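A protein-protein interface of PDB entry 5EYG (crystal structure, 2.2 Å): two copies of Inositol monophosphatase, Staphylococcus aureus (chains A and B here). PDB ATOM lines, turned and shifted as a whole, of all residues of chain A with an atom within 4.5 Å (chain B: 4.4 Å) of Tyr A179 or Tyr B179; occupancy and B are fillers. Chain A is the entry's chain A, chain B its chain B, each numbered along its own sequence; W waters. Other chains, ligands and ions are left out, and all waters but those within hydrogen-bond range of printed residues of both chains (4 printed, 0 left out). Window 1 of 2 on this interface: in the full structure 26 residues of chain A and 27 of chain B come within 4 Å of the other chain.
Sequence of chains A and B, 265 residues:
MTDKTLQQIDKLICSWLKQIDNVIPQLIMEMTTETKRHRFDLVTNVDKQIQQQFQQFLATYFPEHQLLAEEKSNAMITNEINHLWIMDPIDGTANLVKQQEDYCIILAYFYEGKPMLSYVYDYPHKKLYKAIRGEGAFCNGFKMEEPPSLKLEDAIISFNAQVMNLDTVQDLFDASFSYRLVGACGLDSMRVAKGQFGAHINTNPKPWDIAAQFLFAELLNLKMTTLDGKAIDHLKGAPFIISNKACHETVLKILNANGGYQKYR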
ATOM      1  N   ILE A 156      10.789  20.839 -11.635  1.00  0.00           N
ATOM      2  CA  ILE A 156       9.468  21.406 -11.343  1.00  0.00           C
ATOM      3  C   ILE A 156       9.676  22.598 -10.461  1.00  0.00           C
ATOM      4  O   ILE A 156      10.504  22.531  -9.535  1.00  0.00           O
ATOM      5  CB  ILE A 156       8.629  20.411 -10.599  1.00  0.00           C
ATOM      6  CG1 ILE A 156       8.340  19.234 -11.494  1.00  0.00           C
ATOM      7  CG2 ILE A 156       7.348  21.041 -10.089  1.00  0.00           C
ATOM      8  CD1 ILE A 156       7.684  18.091 -10.757  1.00  0.00           C
ATOM      9  N   ILE A 157       8.952  23.675 -10.705  1.00  0.00           N
ATOM     10  CA  ILE A 157       9.046  24.796  -9.745  1.00  0.00           C
ATOM     11  C   ILE A 157       7.746  25.180  -9.148  1.00  0.00           C
ATOM     12  O   ILE A 157       6.708  24.848  -9.682  1.00  0.00           O
ATOM     13  CB  ILE A 157       9.701  26.028 -10.331  1.00  0.00           C
ATOM     14  CG1 ILE A 157       8.934  26.516 -11.523  1.00  0.00           C
ATOM     15  CG2 ILE A 157      11.141  25.679 -10.668  1.00  0.00           C
ATOM     16  CD1 ILE A 157       9.574  27.731 -12.126  1.00  0.00           C
ATOM     17  N   PHE A 159       5.759  28.424  -7.033  1.00  0.00           N
ATOM     18  CA  PHE A 159       5.665  29.824  -6.656  1.00  0.00           C
ATOM     19  C   PHE A 159       4.189  30.191  -6.706  1.00  0.00           C
ATOM     20  O   PHE A 159       3.337  29.427  -7.205  1.00  0.00           O
ATOM     21  CB  PHE A 159       6.491  30.742  -7.597  1.00  0.00           C
ATOM     22  CG  PHE A 159       6.117  30.626  -9.044  1.00  0.00           C
ATOM     23  CD1 PHE A 159       6.735  29.657  -9.870  1.00  0.00           C
ATOM     24  CD2 PHE A 159       5.159  31.465  -9.608  1.00  0.00           C
ATOM     25  CE1 PHE A 159       6.403  29.544 -11.198  1.00  0.00           C
ATOM     26  CE2 PHE A 159       4.855  31.368 -10.948  1.00  0.00           C
ATOM     27  CZ  PHE A 159       5.464  30.382 -11.738  1.00  0.00           C
ATOM     28  N   ALA A 161       1.652  32.279  -8.426  1.00  0.00           N
ATOM     29  CA  ALA A 161       1.528  32.954  -9.754  1.00  0.00           C
ATOM     30  C   ALA A 161       0.623  34.208  -9.671  1.00  0.00           C
ATOM     31  O   ALA A 161       0.718  35.071 -10.521  1.00  0.00           O
ATOM     32  CB  ALA A 161       0.978  32.006 -10.803  1.00  0.00           C
ATOM     33  N   GLN A 162      -0.143  34.330  -8.583  1.00  0.00           N
ATOM     34  CA  GLN A 162      -1.101  35.426  -8.444  1.00  0.00           C
ATOM     35  C   GLN A 162      -0.488  36.735  -7.966  1.00  0.00           C
ATOM     36  O   GLN A 162      -1.168  37.722  -7.952  1.00  0.00           O
ATOM     37  CB  GLN A 162      -2.198  35.059  -7.391  1.00  0.00           C
ATOM     38  CG  GLN A 162      -2.794  33.669  -7.608  1.00  0.00           C
ATOM     39  CD  GLN A 162      -4.037  33.351  -6.792  1.00  0.00           C
ATOM     40  OE1 GLN A 162      -4.119  32.294  -6.197  1.00  0.00           O
ATOM     41  NE2 GLN A 162      -5.005  34.207  -6.808  1.00  0.00           N
ATOM     42  N   PHE A 173       7.127  29.428 -16.529  1.00  0.00           N
ATOM     43  CA  PHE A 173       6.501  28.222 -17.113  1.00  0.00           C
ATOM     44  C   PHE A 173       7.370  27.664 -18.270  1.00  0.00           C
ATOM     45  O   PHE A 173       7.715  26.468 -18.309  1.00  0.00           O
ATOM     46  CB  PHE A 173       5.105  28.514 -17.647  1.00  0.00           C
ATOM     47  CG  PHE A 173       4.074  28.727 -16.615  1.00  0.00           C
ATOM     48  CD1 PHE A 173       4.295  28.425 -15.274  1.00  0.00           C
ATOM     49  CD2 PHE A 173       2.853  29.210 -16.977  1.00  0.00           C
ATOM     50  CE1 PHE A 173       3.296  28.613 -14.333  1.00  0.00           C
ATOM     51  CE2 PHE A 173       1.838  29.401 -16.040  1.00  0.00           C
ATOM     52  CZ  PHE A 173       2.062  29.102 -14.718  1.00  0.00           C
ATOM     53  N   SER A 178       8.021  21.871 -15.296  1.00  0.00           N
ATOM     54  CA  SER A 178       6.604  22.028 -15.030  1.00  0.00           C
ATOM     55  C   SER A 178       6.424  22.851 -13.767  1.00  0.00           C
ATOM     56  O   SER A 178       7.405  23.274 -13.135  1.00  0.00           O
ATOM     57  CB  SER A 178       5.888  20.686 -14.895  1.00  0.00           C
ATOM     58  OG  SER A 178       4.468  20.863 -14.988  1.00  0.00           O
ATOM     59  N   TYR A 179       5.179  23.028 -13.358  1.00  0.00           N
ATOM     60  CA  TYR A 179       4.817  23.890 -12.250  1.00  0.00           C
ATOM     61  C   TYR A 179       3.839  23.140 -11.324  1.00  0.00           C
ATOM     62  O   TYR A 179       2.944  22.406 -11.789  1.00  0.00           O
ATOM     63  CB  TYR A 179       4.200  25.134 -12.837  1.00  0.00           C
ATOM     64  CG  TYR A 179       3.503  25.969 -11.821  1.00  0.00           C
ATOM     65  CD1 TYR A 179       4.203  26.903 -11.062  1.00  0.00           C
ATOM     66  CD2 TYR A 179       2.145  25.813 -11.571  1.00  0.00           C
ATOM     67  CE1 TYR A 179       3.566  27.693 -10.150  1.00  0.00           C
ATOM     68  CE2 TYR A 179       1.501  26.619 -10.624  1.00  0.00           C
ATOM     69  CZ  TYR A 179       2.223  27.562  -9.913  1.00  0.00           C
ATOM     70  OH  TYR A 179       1.630  28.351  -8.925  1.00  0.00           O
ATOM     71  N   ARG A 180       4.095  23.255 -10.020  1.00  0.00           N
ATOM     72  CA  ARG A 180       3.235  22.681  -9.022  1.00  0.00           C
ATOM     73  C   ARG A 180       3.120  23.672  -7.863  1.00  0.00           C
ATOM     74  O   ARG A 180       3.983  24.536  -7.699  1.00  0.00           O
ATOM     75  CB  ARG A 180       3.811  21.355  -8.505  1.00  0.00           C
ATOM     76  CG  ARG A 180       4.033  20.236  -9.515  1.00  0.00           C
ATOM     77  CD  ARG A 180       2.686  19.615  -9.950  1.00  0.00           C
ATOM     78  NE  ARG A 180       2.893  18.495 -10.882  1.00  0.00           N
ATOM     79  CZ  ARG A 180       2.950  18.582 -12.226  1.00  0.00           C
ATOM     80  NH1 ARG A 180       3.155  17.469 -12.922  1.00  0.00           N
ATOM     81  NH2 ARG A 180       2.756  19.710 -12.921  1.00  0.00           N
ATOM     82  N   LEU A 181       2.088  23.501  -7.026  1.00  0.00           N
ATOM     83  CA  LEU A 181       2.041  24.267  -5.807  1.00  0.00           C
ATOM     84  C   LEU A 181       1.352  23.527  -4.679  1.00  0.00           C
ATOM     85  O   LEU A 181       0.216  23.116  -4.778  1.00  0.00           O
ATOM     86  CB  LEU A 181       1.386  25.616  -6.069  1.00  0.00           C
ATOM     87  CG  LEU A 181       1.340  26.572  -4.878  1.00  0.00           C
ATOM     88  CD1 LEU A 181       2.730  26.953  -4.411  1.00  0.00           C
ATOM     89  CD2 LEU A 181       0.539  27.788  -5.241  1.00  0.00           C
ATOM     90  N   ILE B 156     -10.823  26.486  -3.260  1.00  0.00           N
ATOM     91  CA  ILE B 156      -9.511  26.357  -3.931  1.00  0.00           C
ATOM     92  C   ILE B 156      -9.772  25.673  -5.243  1.00  0.00           C
ATOM     93  O   ILE B 156     -10.543  24.690  -5.279  1.00  0.00           O
ATOM     94  CB  ILE B 156      -8.572  25.488  -3.127  1.00  0.00           C
ATOM     95  CG1 ILE B 156      -8.254  26.177  -1.821  1.00  0.00           C
ATOM     96  CG2 ILE B 156      -7.318  25.158  -3.929  1.00  0.00           C
ATOM     97  CD1 ILE B 156      -7.482  25.291  -0.866  1.00  0.00           C
ATOM     98  N   ILE B 157      -9.129  26.130  -6.312  1.00  0.00           N
ATOM     99  CA  ILE B 157      -9.321  25.466  -7.582  1.00  0.00           C
ATOM    100  C   ILE B 157      -7.993  24.976  -8.153  1.00  0.00           C
ATOM    101  O   ILE B 157      -6.930  25.486  -7.788  1.00  0.00           O
ATOM    102  CB  ILE B 157     -10.069  26.563  -8.360  1.00  0.00           C
ATOM    103  CG1 ILE B 157     -11.000  25.974  -9.338  1.00  0.00           C
ATOM    104  CG2 ILE B 157      -9.138  27.653  -8.941  1.00  0.00           C
ATOM    105  CD1 ILE B 157     -10.351  25.794 -10.674  1.00  0.00           C
ATOM    106  N   PHE B 159      -6.119  23.527 -11.807  1.00  0.00           N
ATOM    107  CA  PHE B 159      -6.111  23.368 -13.253  1.00  0.00           C
ATOM    108  C   PHE B 159      -4.687  23.566 -13.704  1.00  0.00           C
ATOM    109  O   PHE B 159      -3.802  23.989 -12.944  1.00  0.00           O
ATOM    110  CB  PHE B 159      -7.066  24.368 -13.946  1.00  0.00           C
ATOM    111  CG  PHE B 159      -6.793  25.800 -13.599  1.00  0.00           C
ATOM    112  CD1 PHE B 159      -7.368  26.392 -12.482  1.00  0.00           C
ATOM    113  CD2 PHE B 159      -5.913  26.546 -14.366  1.00  0.00           C
ATOM    114  CE1 PHE B 159      -7.087  27.701 -12.161  1.00  0.00           C
ATOM    115  CE2 PHE B 159      -5.664  27.860 -14.073  1.00  0.00           C
ATOM    116  CZ  PHE B 159      -6.223  28.434 -12.962  1.00  0.00           C
ATOM    117  N   ALA B 161      -2.391  25.753 -15.611  1.00  0.00           N
ATOM    118  CA  ALA B 161      -2.388  27.159 -16.046  1.00  0.00           C
ATOM    119  C   ALA B 161      -1.610  27.335 -17.351  1.00  0.00           C
ATOM    120  O   ALA B 161      -1.807  28.322 -18.073  1.00  0.00           O
ATOM    121  CB  ALA B 161      -1.827  28.090 -14.987  1.00  0.00           C
ATOM    122  N   GLN B 162      -0.757  26.373 -17.687  1.00  0.00           N
ATOM    123  CA  GLN B 162       0.145  26.518 -18.856  1.00  0.00           C
ATOM    124  C   GLN B 162      -0.533  26.204 -20.208  1.00  0.00           C
ATOM    125  O   GLN B 162       0.054  26.384 -21.243  1.00  0.00           O
ATOM    126  CB  GLN B 162       1.329  25.518 -18.756  1.00  0.00           C
ATOM    127  CG  GLN B 162       2.034  25.556 -17.404  1.00  0.00           C
ATOM    128  CD  GLN B 162       3.323  24.768 -17.329  1.00  0.00           C
ATOM    129  OE1 GLN B 162       3.493  23.986 -16.431  1.00  0.00           O
ATOM    130  NE2 GLN B 162       4.223  24.986 -18.236  1.00  0.00           N
ATOM    131  N   PHE B 173      -8.113  32.900 -11.078  1.00  0.00           N
ATOM    132  CA  PHE B 173      -7.399  33.309  -9.860  1.00  0.00           C
ATOM    133  C   PHE B 173      -8.270  34.286  -9.073  1.00  0.00           C
ATOM    134  O   PHE B 173      -8.510  34.110  -7.880  1.00  0.00           O
ATOM    135  CB  PHE B 173      -6.068  33.981 -10.190  1.00  0.00           C
ATOM    136  CG  PHE B 173      -4.992  33.055 -10.645  1.00  0.00           C
ATOM    137  CD1 PHE B 173      -5.091  31.694 -10.506  1.00  0.00           C
ATOM    138  CD2 PHE B 173      -3.827  33.582 -11.192  1.00  0.00           C
ATOM    139  CE1 PHE B 173      -4.053  30.880 -10.930  1.00  0.00           C
ATOM    140  CE2 PHE B 173      -2.777  32.767 -11.604  1.00  0.00           C
ATOM    141  CZ  PHE B 173      -2.896  31.417 -11.474  1.00  0.00           C
ATOM    142  N   SER B 178      -8.337  30.368  -3.721  1.00  0.00           N
ATOM    143  CA  SER B 178      -6.918  30.197  -4.043  1.00  0.00           C
ATOM    144  C   SER B 178      -6.722  29.114  -5.110  1.00  0.00           C
ATOM    145  O   SER B 178      -7.663  28.527  -5.615  1.00  0.00           O
ATOM    146  CB  SER B 178      -6.119  29.838  -2.793  1.00  0.00           C
ATOM    147  OG  SER B 178      -4.721  30.020  -3.016  1.00  0.00           O
ATOM    148  N   TYR B 179      -5.456  28.881  -5.455  1.00  0.00           N
ATOM    149  CA  TYR B 179      -5.095  27.976  -6.538  1.00  0.00           C
ATOM    150  C   TYR B 179      -4.062  26.990  -5.998  1.00  0.00           C
ATOM    151  O   TYR B 179      -3.086  27.376  -5.279  1.00  0.00           O
ATOM    152  CB  TYR B 179      -4.593  28.799  -7.722  1.00  0.00           C
ATOM    153  CG  TYR B 179      -3.910  27.991  -8.780  1.00  0.00           C
ATOM    154  CD1 TYR B 179      -4.632  27.352  -9.765  1.00  0.00           C
ATOM    155  CD2 TYR B 179      -2.553  27.762  -8.734  1.00  0.00           C
ATOM    156  CE1 TYR B 179      -4.020  26.534 -10.717  1.00  0.00           C
ATOM    157  CE2 TYR B 179      -1.934  26.939  -9.658  1.00  0.00           C
ATOM    158  CZ  TYR B 179      -2.678  26.333 -10.667  1.00  0.00           C
ATOM    159  OH  TYR B 179      -2.065  25.560 -11.622  1.00  0.00           O
ATOM    160  N   ARG B 180      -4.244  25.722  -6.363  1.00  0.00           N
ATOM    161  CA  ARG B 180      -3.287  24.667  -5.987  1.00  0.00           C
ATOM    162  C   ARG B 180      -3.205  23.707  -7.153  1.00  0.00           C
ATOM    163  O   ARG B 180      -4.105  23.664  -8.036  1.00  0.00           O
ATOM    164  CB  ARG B 180      -3.727  23.896  -4.762  1.00  0.00           C
ATOM    165  CG  ARG B 180      -3.968  24.635  -3.453  1.00  0.00           C
ATOM    166  CD  ARG B 180      -2.871  24.772  -2.363  1.00  0.00           C
ATOM    167  NE  ARG B 180      -2.594  26.089  -2.415  1.00  0.00           N
ATOM    168  CZ  ARG B 180      -2.993  27.150  -1.779  1.00  0.00           C
ATOM    169  NH1 ARG B 180      -3.209  27.311  -0.485  1.00  0.00           N
ATOM    170  NH2 ARG B 180      -2.671  28.175  -2.511  1.00  0.00           N
ATOM    171  N   LEU B 181      -2.145  22.917  -7.220  1.00  0.00           N
ATOM    172  CA  LEU B 181      -2.078  21.859  -8.256  1.00  0.00           C
ATOM    173  C   LEU B 181      -1.236  20.697  -7.765  1.00  0.00           C
ATOM    174  O   LEU B 181      -0.058  20.832  -7.454  1.00  0.00           O
ATOM    175  CB  LEU B 181      -1.520  22.383  -9.568  1.00  0.00           C
ATOM    176  CG  LEU B 181      -1.449  21.388 -10.720  1.00  0.00           C
ATOM    177  CD1 LEU B 181      -2.852  20.906 -11.088  1.00  0.00           C
ATOM    178  CD2 LEU B 181      -0.731  21.978 -11.918  1.00  0.00           C
HETATM  179  O   HOH W   1      -7.276  31.941  -6.620  1.00  0.00           O
HETATM  180  O   HOH W   2       1.495  22.947 -14.325  1.00  0.00           O
HETATM  181  O   HOH W   3       6.694  24.946 -16.187  1.00  0.00           O
HETATM  182  O   HOH W   4      -2.014  30.157  -5.500  1.00  0.00           O
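The backbone carbonyl oxygen (O) of Leu A181 is in hydrogen-bond range of the backbone NH (N) of Leu B181 (3.4 Å).
The side-chain hydroxyl of Ser A178 is in hydrogen-bond range of the guanidinium group of Arg A180, at 2.9 Å. OH of Tyr A179 lies within hydrogen-bond range of O of Phe A159 (2.7 Å). The backbone carbonyl oxygen (O) of Phe B159 is in hydrogen-bond range of the side-chain hydroxyl (OH) of Tyr B179, at 2.7 Å. The backbone carbonyl oxygen of Ile A157 sits at hydrogen-bond distance from the backbone NH of Arg A180 (3.1 Å). O of Ser A178 sits at hydrogen-bond distance from N of Ile A157, at 2.9 Å. OG of Ser B178 lies within hydrogen-bond range of NH2 of Arg B180, 2.8 Å away.
Among the printed residues, pairs that only touch across the chains: Gln A162 with Phe B173 (3.6 Å), Ser A178 with Gln B162 (3.6 Å), Tyr A179 with Tyr B179 (3.6 Å), Tyr A179 with Gln B162 (3.6 Å), Leu A181 with Tyr B179 (3.6 Å), Phe A173 with Gln B162 (3.7 Å), Tyr A179 with Leu B181 (3.7 Å), Gln A162 with Tyr B179 (3.7 Å), Arg A180 with Leu B181 (3.9 Å), Ala A161 with Phe B173 (3.9 Å) and Gln A162 with Ser B178 (3.96 Å).
Ile A157 touches none of the printed residues of chain B. Of the printed residues of chain B, Gln A162 touches Phe B173, Ser B178 and Tyr B179. Of the printed residues of chain B, Phe A173 touches Gln B162 (3.7 Å). Of the printed residues of chain B, Ser A178 touches Gln B162. Of the printed residues of chain B, Tyr A179 touches Gln B162, Tyr B179 and Leu B181. Of the printed residues of chain B, Leu A181 touches Tyr B179 and Leu B181. Ile B157 touches none of the printed residues of chain A. Printed residues of chain A within 4 Å of Gln B162: Phe A173 (3.7 Å), Ser A178 (3.6 Å) and Tyr A179 (3.6 Å).
Of the 10 printed residues of chain B, 5 touch a printed residue of chain A. Hydrophobic or aromatic side chains of chain B that line the printed part of chain A: Phe B173, Tyr B179 and Leu B181. Hydrophobic or aromatic side chains of chain A that line the printed part of chain B: Ala A161, Phe A173, Tyr A179 and Leu A181.
Gln A162 touches Ser B178, and with the chains exchanged Ser A178 touches Gln B162. Gln A162 touches Tyr B179, and with the chains exchanged Tyr A179 touches Gln B162. Tyr A179 touches Leu B181, and with the chains exchanged Leu A181 touches Tyr B179. Leu A181 touches its own counterpart, Leu B181.
Water W1 lies within hydrogen-bond range of O of Phe B173 (2.8 Å), OE1 of Gln A162 (3.2 Å) and N of Ser B178 (3.5 Å). Water W3 lies within hydrogen-bond range of O of Phe A173 (2.8 Å), NE2 of Gln B162 (3.2 Å) and N of Ser A178 (3.5 Å). Water W2 lies within hydrogen-bond range of the backbone carbonyl oxygen of Tyr A179 (3.0 Å) and the side-chain amide oxygen of Gln B162 (3.1 Å). Water W4 lies within hydrogen-bond range of O of Tyr B179 and OE1 of Gln A162.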
